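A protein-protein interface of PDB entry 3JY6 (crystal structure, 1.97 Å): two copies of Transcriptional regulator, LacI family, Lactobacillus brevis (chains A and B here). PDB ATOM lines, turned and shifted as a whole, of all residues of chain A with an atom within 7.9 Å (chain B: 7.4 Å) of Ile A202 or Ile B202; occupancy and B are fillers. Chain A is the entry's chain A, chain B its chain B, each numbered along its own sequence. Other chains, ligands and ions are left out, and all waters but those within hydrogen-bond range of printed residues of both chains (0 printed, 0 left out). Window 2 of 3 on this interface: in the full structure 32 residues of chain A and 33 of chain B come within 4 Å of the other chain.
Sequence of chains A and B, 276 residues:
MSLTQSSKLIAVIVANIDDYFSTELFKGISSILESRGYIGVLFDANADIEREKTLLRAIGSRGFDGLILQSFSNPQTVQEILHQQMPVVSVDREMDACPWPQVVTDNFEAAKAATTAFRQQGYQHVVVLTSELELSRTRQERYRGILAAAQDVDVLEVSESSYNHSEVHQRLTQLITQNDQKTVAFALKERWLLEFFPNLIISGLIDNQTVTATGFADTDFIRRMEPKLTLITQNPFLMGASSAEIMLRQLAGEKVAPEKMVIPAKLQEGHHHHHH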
ATOM      1  N   PHE A 197      15.051 -12.644 -29.829  1.00  0.00           N
ATOM      2  CA  PHE A 197      13.783 -13.082 -29.237  1.00  0.00           C
ATOM      3  C   PHE A 197      13.683 -13.107 -27.704  1.00  0.00           C
ATOM      4  O   PHE A 197      12.608 -12.844 -27.148  1.00  0.00           O
ATOM      5  CB  PHE A 197      13.388 -14.463 -29.791  1.00  0.00           C
ATOM      6  CG  PHE A 197      12.943 -14.454 -31.241  1.00  0.00           C
ATOM      7  CD1 PHE A 197      13.079 -13.312 -32.041  1.00  0.00           C
ATOM      8  CD2 PHE A 197      12.399 -15.601 -31.812  1.00  0.00           C
ATOM      9  CE1 PHE A 197      12.678 -13.318 -33.388  1.00  0.00           C
ATOM     10  CE2 PHE A 197      11.995 -15.622 -33.151  1.00  0.00           C
ATOM     11  CZ  PHE A 197      12.136 -14.475 -33.944  1.00  0.00           C
ATOM     12  N   PRO A 198      14.780 -13.443 -26.998  1.00  0.00           N
ATOM     13  CA  PRO A 198      14.709 -13.476 -25.530  1.00  0.00           C
ATOM     14  C   PRO A 198      14.183 -12.213 -24.842  1.00  0.00           C
ATOM     15  O   PRO A 198      13.366 -12.304 -23.926  1.00  0.00           O
ATOM     16  CB  PRO A 198      16.141 -13.812 -25.128  1.00  0.00           C
ATOM     17  CG  PRO A 198      16.540 -14.776 -26.194  1.00  0.00           C
ATOM     18  CD  PRO A 198      16.027 -14.087 -27.467  1.00  0.00           C
ATOM     19  N   ASN A 199      14.645 -11.037 -25.264  1.00  0.00           N
ATOM     20  CA  ASN A 199      14.173  -9.802 -24.640  1.00  0.00           C
ATOM     21  C   ASN A 199      12.723  -9.500 -25.006  1.00  0.00           C
ATOM     22  O   ASN A 199      12.016  -8.830 -24.259  1.00  0.00           O
ATOM     23  CB  ASN A 199      15.072  -8.622 -25.018  1.00  0.00           C
ATOM     24  CG  ASN A 199      16.328  -8.550 -24.168  1.00  0.00           C
ATOM     25  OD1 ASN A 199      16.684  -7.487 -23.666  1.00  0.00           O
ATOM     26  ND2 ASN A 199      17.004  -9.682 -24.005  1.00  0.00           N
ATOM     27  N   LEU A 200      12.274  -9.988 -26.158  1.00  0.00           N
ATOM     28  CA  LEU A 200      10.889  -9.774 -26.554  1.00  0.00           C
ATOM     29  C   LEU A 200       9.974 -10.708 -25.744  1.00  0.00           C
ATOM     30  O   LEU A 200       8.765 -10.487 -25.651  1.00  0.00           O
ATOM     31  CB  LEU A 200      10.724 -10.003 -28.061  1.00  0.00           C
ATOM     32  CG  LEU A 200      10.916  -8.754 -28.936  1.00  0.00           C
ATOM     33  CD1 LEU A 200      12.241  -8.063 -28.608  1.00  0.00           C
ATOM     34  CD2 LEU A 200      10.852  -9.148 -30.405  1.00  0.00           C
ATOM     35  N   ILE A 201      10.556 -11.744 -25.146  1.00  0.00           N
ATOM     36  CA  ILE A 201       9.787 -12.676 -24.327  1.00  0.00           C
ATOM     37  C   ILE A 201       9.783 -12.140 -22.905  1.00  0.00           C
ATOM     38  O   ILE A 201       8.818 -12.298 -22.165  1.00  0.00           O
ATOM     39  CB  ILE A 201      10.417 -14.086 -24.296  1.00  0.00           C
ATOM     40  CG1 ILE A 201      10.359 -14.715 -25.687  1.00  0.00           C
ATOM     41  CG2 ILE A 201       9.690 -14.955 -23.262  1.00  0.00           C
ATOM     42  CD1 ILE A 201      11.018 -16.075 -25.790  1.00  0.00           C
ATOM     43  N   ILE A 202      10.885 -11.500 -22.535  1.00  0.00           N
ATOM     44  CA  ILE A 202      11.024 -10.939 -21.205  1.00  0.00           C
ATOM     45  C   ILE A 202      10.330  -9.581 -21.089  1.00  0.00           C
ATOM     46  O   ILE A 202       9.833  -9.232 -20.021  1.00  0.00           O
ATOM     47  CB  ILE A 202      12.523 -10.846 -20.833  1.00  0.00           C
ATOM     48  CG1 ILE A 202      13.054 -12.265 -20.588  1.00  0.00           C
ATOM     49  CG2 ILE A 202      12.726  -9.960 -19.609  1.00  0.00           C
ATOM     50  CD1 ILE A 202      14.562 -12.378 -20.492  1.00  0.00           C
ATOM     51  N   SER A 203      10.272  -8.826 -22.185  1.00  0.00           N
ATOM     52  CA  SER A 203       9.619  -7.517 -22.157  1.00  0.00           C
ATOM     53  C   SER A 203       8.104  -7.658 -22.284  1.00  0.00           C
ATOM     54  O   SER A 203       7.366  -6.706 -22.047  1.00  0.00           O
ATOM     55  CB  SER A 203      10.147  -6.621 -23.284  1.00  0.00           C
ATOM     56  OG  SER A 203       9.771  -7.108 -24.555  1.00  0.00           O
ATOM     57  N   GLY A 204       7.641  -8.846 -22.667  1.00  0.00           N
ATOM     58  CA  GLY A 204       6.211  -9.070 -22.792  1.00  0.00           C
ATOM     59  C   GLY A 204       5.626  -8.988 -24.191  1.00  0.00           C
ATOM     60  O   GLY A 204       4.451  -9.309 -24.402  1.00  0.00           O
ATOM     61  N   LEU A 205       6.430  -8.570 -25.163  1.00  0.00           N
ATOM     62  CA  LEU A 205       5.927  -8.460 -26.529  1.00  0.00           C
ATOM     63  C   LEU A 205       5.419  -9.803 -27.049  1.00  0.00           C
ATOM     64  O   LEU A 205       4.312  -9.892 -27.574  1.00  0.00           O
ATOM     65  CB  LEU A 205       7.010  -7.906 -27.455  1.00  0.00           C
ATOM     66  CG  LEU A 205       6.584  -7.642 -28.901  1.00  0.00           C
ATOM     67  CD1 LEU A 205       5.409  -6.672 -28.959  1.00  0.00           C
ATOM     68  CD2 LEU A 205       7.756  -7.074 -29.653  1.00  0.00           C
ATOM     69  N   ILE A 206       6.232 -10.845 -26.912  1.00  0.00           N
ATOM     70  CA  ILE A 206       5.836 -12.180 -27.351  1.00  0.00           C
ATOM     71  C   ILE A 206       4.996 -12.795 -26.228  1.00  0.00           C
ATOM     72  O   ILE A 206       5.537 -13.174 -25.187  1.00  0.00           O
ATOM     73  CB  ILE A 206       7.083 -13.067 -27.621  1.00  0.00           C
ATOM     74  CG1 ILE A 206       7.855 -12.526 -28.836  1.00  0.00           C
ATOM     75  CG2 ILE A 206       6.661 -14.509 -27.870  1.00  0.00           C
ATOM     76  CD1 ILE A 206       9.218 -13.158 -29.038  1.00  0.00           C
ATOM     77  N   ARG A 224      13.370 -24.269 -23.761  1.00  0.00           N
ATOM     78  CA  ARG A 224      12.942 -23.888 -22.447  1.00  0.00           C
ATOM     79  C   ARG A 224      12.888 -22.415 -22.276  1.00  0.00           C
ATOM     80  O   ARG A 224      13.685 -21.887 -21.547  1.00  0.00           O
ATOM     81  CB  ARG A 224      13.985 -24.335 -21.469  1.00  0.00           C
ATOM     82  CG  ARG A 224      14.793 -25.432 -22.024  1.00  0.00           C
ATOM     83  CD  ARG A 224      15.806 -25.970 -21.120  1.00  0.00           C
ATOM     84  NE  ARG A 224      16.202 -27.274 -21.594  1.00  0.00           N
ATOM     85  CZ  ARG A 224      15.510 -28.385 -21.392  1.00  0.00           C
ATOM     86  NH1 ARG A 224      14.390 -28.341 -20.700  1.00  0.00           N
ATOM     87  NH2 ARG A 224      15.934 -29.520 -21.875  1.00  0.00           N
ATOM     88  N   MET A 225      11.946 -21.723 -22.889  1.00  0.00           N
ATOM     89  CA  MET A 225      11.763 -20.320 -22.511  1.00  0.00           C
ATOM     90  C   MET A 225      10.356 -20.029 -22.005  1.00  0.00           C
ATOM     91  O   MET A 225      10.170 -19.811 -20.813  1.00  0.00           O
ATOM     92  CB  MET A 225      12.254 -19.303 -23.561  1.00  0.00           C
ATOM     93  CG  MET A 225      13.792 -19.144 -23.576  1.00  0.00           C
ATOM     94  SD  MET A 225      14.464 -17.486 -23.533  1.00  0.00           S
ATOM     95  CE  MET A 225      14.352 -17.134 -21.876  1.00  0.00           C
ATOM     96  N   LYS A 228       7.213 -21.721 -23.402  1.00  0.00           N
ATOM     97  CA  LYS A 228       7.299 -22.731 -24.538  1.00  0.00           C
ATOM     98  C   LYS A 228       6.958 -22.423 -26.036  1.00  0.00           C
ATOM     99  O   LYS A 228       5.831 -22.435 -26.734  1.00  0.00           O
ATOM    100  CB  LYS A 228       7.116 -24.219 -24.249  1.00  0.00           C
ATOM    101  CG  LYS A 228       7.416 -24.960 -25.491  1.00  0.00           C
ATOM    102  CD  LYS A 228       8.247 -26.094 -25.039  1.00  0.00           C
ATOM    103  CE  LYS A 228       7.515 -27.355 -25.368  1.00  0.00           C
ATOM    104  NZ  LYS A 228       6.748 -27.849 -24.184  1.00  0.00           N
ATOM    105  N   PHE B 197      18.764 -20.292 -15.781  1.00  0.00           N
ATOM    106  CA  PHE B 197      18.499 -18.905 -15.417  1.00  0.00           C
ATOM    107  C   PHE B 197      17.469 -18.165 -16.280  1.00  0.00           C
ATOM    108  O   PHE B 197      16.679 -17.383 -15.753  1.00  0.00           O
ATOM    109  CB  PHE B 197      19.820 -18.126 -15.344  1.00  0.00           C
ATOM    110  CG  PHE B 197      20.757 -18.608 -14.255  1.00  0.00           C
ATOM    111  CD1 PHE B 197      20.367 -19.607 -13.360  1.00  0.00           C
ATOM    112  CD2 PHE B 197      22.037 -18.062 -14.125  1.00  0.00           C
ATOM    113  CE1 PHE B 197      21.241 -20.057 -12.353  1.00  0.00           C
ATOM    114  CE2 PHE B 197      22.917 -18.503 -13.124  1.00  0.00           C
ATOM    115  CZ  PHE B 197      22.518 -19.501 -12.237  1.00  0.00           C
ATOM    116  N   PRO B 198      17.443 -18.409 -17.604  1.00  0.00           N
ATOM    117  CA  PRO B 198      16.448 -17.690 -18.416  1.00  0.00           C
ATOM    118  C   PRO B 198      15.031 -17.806 -17.836  1.00  0.00           C
ATOM    119  O   PRO B 198      14.378 -16.801 -17.544  1.00  0.00           O
ATOM    120  CB  PRO B 198      16.575 -18.362 -19.782  1.00  0.00           C
ATOM    121  CG  PRO B 198      18.024 -18.745 -19.826  1.00  0.00           C
ATOM    122  CD  PRO B 198      18.239 -19.325 -18.442  1.00  0.00           C
ATOM    123  N   ASN B 199      14.561 -19.039 -17.669  1.00  0.00           N
ATOM    124  CA  ASN B 199      13.230 -19.280 -17.120  1.00  0.00           C
ATOM    125  C   ASN B 199      13.029 -18.591 -15.774  1.00  0.00           C
ATOM    126  O   ASN B 199      11.954 -18.056 -15.494  1.00  0.00           O
ATOM    127  CB  ASN B 199      12.988 -20.778 -16.957  1.00  0.00           C
ATOM    128  CG  ASN B 199      12.190 -21.370 -18.097  1.00  0.00           C
ATOM    129  OD1 ASN B 199      12.624 -21.377 -19.248  1.00  0.00           O
ATOM    130  ND2 ASN B 199      11.005 -21.870 -17.778  1.00  0.00           N
ATOM    131  N   LEU B 200      14.062 -18.614 -14.939  1.00  0.00           N
ATOM    132  CA  LEU B 200      13.976 -17.991 -13.629  1.00  0.00           C
ATOM    133  C   LEU B 200      13.830 -16.478 -13.768  1.00  0.00           C
ATOM    134  O   LEU B 200      13.270 -15.828 -12.888  1.00  0.00           O
ATOM    135  CB  LEU B 200      15.205 -18.341 -12.776  1.00  0.00           C
ATOM    136  CG  LEU B 200      15.392 -19.805 -12.362  1.00  0.00           C
ATOM    137  CD1 LEU B 200      16.672 -19.936 -11.539  1.00  0.00           C
ATOM    138  CD2 LEU B 200      14.206 -20.277 -11.552  1.00  0.00           C
ATOM    139  N   ILE B 201      14.332 -15.916 -14.868  1.00  0.00           N
ATOM    140  CA  ILE B 201      14.198 -14.476 -15.092  1.00  0.00           C
ATOM    141  C   ILE B 201      12.741 -14.189 -15.462  1.00  0.00           C
ATOM    142  O   ILE B 201      12.128 -13.262 -14.938  1.00  0.00           O
ATOM    143  CB  ILE B 201      15.125 -13.968 -16.228  1.00  0.00           C
ATOM    144  CG1 ILE B 201      16.587 -14.003 -15.764  1.00  0.00           C
ATOM    145  CG2 ILE B 201      14.743 -12.544 -16.614  1.00  0.00           C
ATOM    146  CD1 ILE B 201      17.600 -13.712 -16.858  1.00  0.00           C
ATOM    147  N   ILE B 202      12.184 -15.004 -16.351  1.00  0.00           N
ATOM    148  CA  ILE B 202      10.799 -14.828 -16.762  1.00  0.00           C
ATOM    149  C   ILE B 202       9.817 -15.071 -15.608  1.00  0.00           C
ATOM    150  O   ILE B 202       8.881 -14.292 -15.413  1.00  0.00           O
ATOM    151  CB  ILE B 202      10.455 -15.765 -17.936  1.00  0.00           C
ATOM    152  CG1 ILE B 202      11.380 -15.455 -19.114  1.00  0.00           C
ATOM    153  CG2 ILE B 202       8.992 -15.572 -18.353  1.00  0.00           C
ATOM    154  CD1 ILE B 202      11.581 -16.588 -20.055  1.00  0.00           C
ATOM    155  N   SER B 203      10.028 -16.135 -14.833  1.00  0.00           N
ATOM    156  CA  SER B 203       9.122 -16.431 -13.726  1.00  0.00           C
ATOM    157  C   SER B 203       9.199 -15.353 -12.650  1.00  0.00           C
ATOM    158  O   SER B 203       8.303 -15.239 -11.812  1.00  0.00           O
ATOM    159  CB  SER B 203       9.431 -17.803 -13.115  1.00  0.00           C
ATOM    160  OG  SER B 203      10.527 -17.723 -12.225  1.00  0.00           O
ATOM    161  N   GLY B 204      10.276 -14.570 -12.668  1.00  0.00           N
ATOM    162  CA  GLY B 204      10.427 -13.495 -11.700  1.00  0.00           C
ATOM    163  C   GLY B 204      11.184 -13.795 -10.418  1.00  0.00           C
ATOM    164  O   GLY B 204      11.337 -12.906  -9.579  1.00  0.00           O
ATOM    165  N   LEU B 205      11.654 -15.028 -10.244  1.00  0.00           N
ATOM    166  CA  LEU B 205      12.402 -15.379  -9.038  1.00  0.00           C
ATOM    167  C   LEU B 205      13.654 -14.492  -8.961  1.00  0.00           C
ATOM    168  O   LEU B 205      14.009 -13.980  -7.898  1.00  0.00           O
ATOM    169  CB  LEU B 205      12.797 -16.858  -9.082  1.00  0.00           C
ATOM    170  CG  LEU B 205      13.091 -17.586  -7.763  1.00  0.00           C
ATOM    171  CD1 LEU B 205      11.814 -17.683  -6.942  1.00  0.00           C
ATOM    172  CD2 LEU B 205      13.610 -18.989  -8.050  1.00  0.00           C
ATOM    173  N   ILE B 206      14.312 -14.318 -10.105  1.00  0.00           N
ATOM    174  CA  ILE B 206      15.505 -13.488 -10.205  1.00  0.00           C
ATOM    175  C   ILE B 206      15.043 -12.063 -10.485  1.00  0.00           C
ATOM    176  O   ILE B 206      14.859 -11.675 -11.642  1.00  0.00           O
ATOM    177  CB  ILE B 206      16.420 -13.970 -11.360  1.00  0.00           C
ATOM    178  CG1 ILE B 206      16.972 -15.360 -11.033  1.00  0.00           C
ATOM    179  CG2 ILE B 206      17.556 -12.981 -11.586  1.00  0.00           C
ATOM    180  CD1 ILE B 206      17.807 -15.974 -12.132  1.00  0.00           C
ATOM    181  N   ILE B 222      23.539 -13.750 -23.579  1.00  0.00           N
ATOM    182  CA  ILE B 222      22.818 -13.967 -22.271  1.00  0.00           C
ATOM    183  C   ILE B 222      22.620 -12.656 -21.577  1.00  0.00           C
ATOM    184  O   ILE B 222      21.632 -12.458 -20.841  1.00  0.00           O
ATOM    185  CB  ILE B 222      23.599 -14.644 -21.178  1.00  0.00           C
ATOM    186  CG1 ILE B 222      24.990 -14.962 -21.702  1.00  0.00           C
ATOM    187  CG2 ILE B 222      22.740 -15.735 -20.564  1.00  0.00           C
ATOM    188  CD1 ILE B 222      25.533 -16.292 -21.210  1.00  0.00           C
ATOM    189  N   ARG B 224      22.150  -9.793 -22.723  1.00  0.00           N
ATOM    190  CA  ARG B 224      21.132  -8.904 -23.158  1.00  0.00           C
ATOM    191  C   ARG B 224      19.742  -9.221 -22.663  1.00  0.00           C
ATOM    192  O   ARG B 224      18.830  -8.456 -22.938  1.00  0.00           O
ATOM    193  CB  ARG B 224      21.222  -8.756 -24.674  1.00  0.00           C
ATOM    194  CG  ARG B 224      21.908  -9.901 -25.386  1.00  0.00           C
ATOM    195  CD  ARG B 224      21.742  -9.720 -26.883  1.00  0.00           C
ATOM    196  NE  ARG B 224      22.485  -8.569 -27.387  1.00  0.00           N
ATOM    197  CZ  ARG B 224      23.621  -8.662 -28.072  1.00  0.00           C
ATOM    198  NH1 ARG B 224      24.143  -9.855 -28.336  1.00  0.00           N
ATOM    199  NH2 ARG B 224      24.243  -7.565 -28.489  1.00  0.00           N
ATOM    200  N   MET B 225      19.561 -10.302 -21.904  1.00  0.00           N
ATOM    201  CA  MET B 225      18.220 -10.606 -21.387  1.00  0.00           C
ATOM    202  C   MET B 225      17.841  -9.644 -20.258  1.00  0.00           C
ATOM    203  O   MET B 225      18.703  -9.013 -19.641  1.00  0.00           O
ATOM    204  CB  MET B 225      18.134 -12.053 -20.872  1.00  0.00           C
ATOM    205  CG  MET B 225      17.973 -13.098 -21.983  1.00  0.00           C
ATOM    206  SD  MET B 225      17.306 -14.683 -21.390  1.00  0.00           S
ATOM    207  CE  MET B 225      18.717 -15.736 -21.542  1.00  0.00           C
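The side-chain amide nitrogen of Asn A199 sits at hydrogen-bond distance from the backbone carbonyl oxygen of Arg B224 (2.4 Å). The backbone NH of Met B225 sits close to the side-chain amide nitrogen of Asn A199. The backbone carbonyl oxygen (O) of Arg A224 sits close to the side-chain amide oxygen (OD1) of Asn B199 (2.6 Å). The backbone carbonyl oxygen (O) of Met A225 sits close to the side-chain amide oxygen (OD1) of Asn B199 (3.3 Å).
The backbone carbonyl oxygen (O) of Asn A199 is in hydrogen-bond range of the side-chain hydroxyl (OG) of Ser A203, 2.8 Å away.
Pro A198 touches Met B225. Ile A202 touches Ile B201 (CD1 to CG2, 3.9 Å). Ile B202 touches Ile A202. Ile A202 touches Met B225 (CD1 to CB, 3.6 Å). CE of Met A225 touches CB of Pro B198, 3.3 Å away. Ile B202 touches Met A225 (CD1 to CE, 3.4 Å). Met A225 touches Met B225.
Printed residues of chain B within 4 Å of Asn A199: Arg B224 (2.4 Å) and Met B225 (3.0 Å). Of chain B, only Ile B201 (3.9 Å), Ile B202 (3.9 Å) and Met B225 (3.6 Å) come within 4 Å of Ile A202. Gly A204 touches none of the printed residues of chain B. Leu A205 touches none of the printed residues of chain B. Printed residues of chain B within 4 Å of Arg A224: Asn B199. Of the printed residues of chain A, Pro B198 touches Met A225. Of the printed residues of chain A, Ile B201 touches Ile A202. Of chain A, only Ile A202 and Met A225 come within 4 Å of Ile B202. Of the printed residues of chain A, Met B225 touches Pro A198 (3.7 Å), Asn A199 (3.0 Å), Ile A202 (3.6 Å) and Met A225 (3.9 Å). The nearest printed residue of chain A that does not touch Met B225 is Phe A197 (7.2 Å).
Printed residues of chain A that touch a printed residue of chain B: Pro A198, Asn A199, Ile A202, Arg A224 and Met A225. Hydrophobic or aromatic side chains of chain A that line the printed part of chain B: Pro A198, Ile A202 and Met A225. Of the 13 printed residues of chain B, 6 touch a printed residue of chain A. Hydrophobic or aromatic side chains of chain B that line the printed part of chain A: Pro B198, Ile B201, Ile B202 and Met B225. Among the printed residues, no Asp or Glu carboxylate lies within 4 Å of a Lys or Arg side-chain nitrogen of the other chain.
Pro A198 touches Met B225, and with the chains exchanged Met A225 touches Pro B198. Asn A199 touches Arg B224, and with the chains exchanged Arg A224 touches Asn B199. Ile A202 touches Ile B201, but with the chains exchanged Ile A201 does not touch Ile B202 (4.1 Å). Ile A202 touches its own counterpart, Ile B202. Of the 11 pairs that touch across the chains among the printed residues, 10 have their exchanged pair printed and touching as well.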
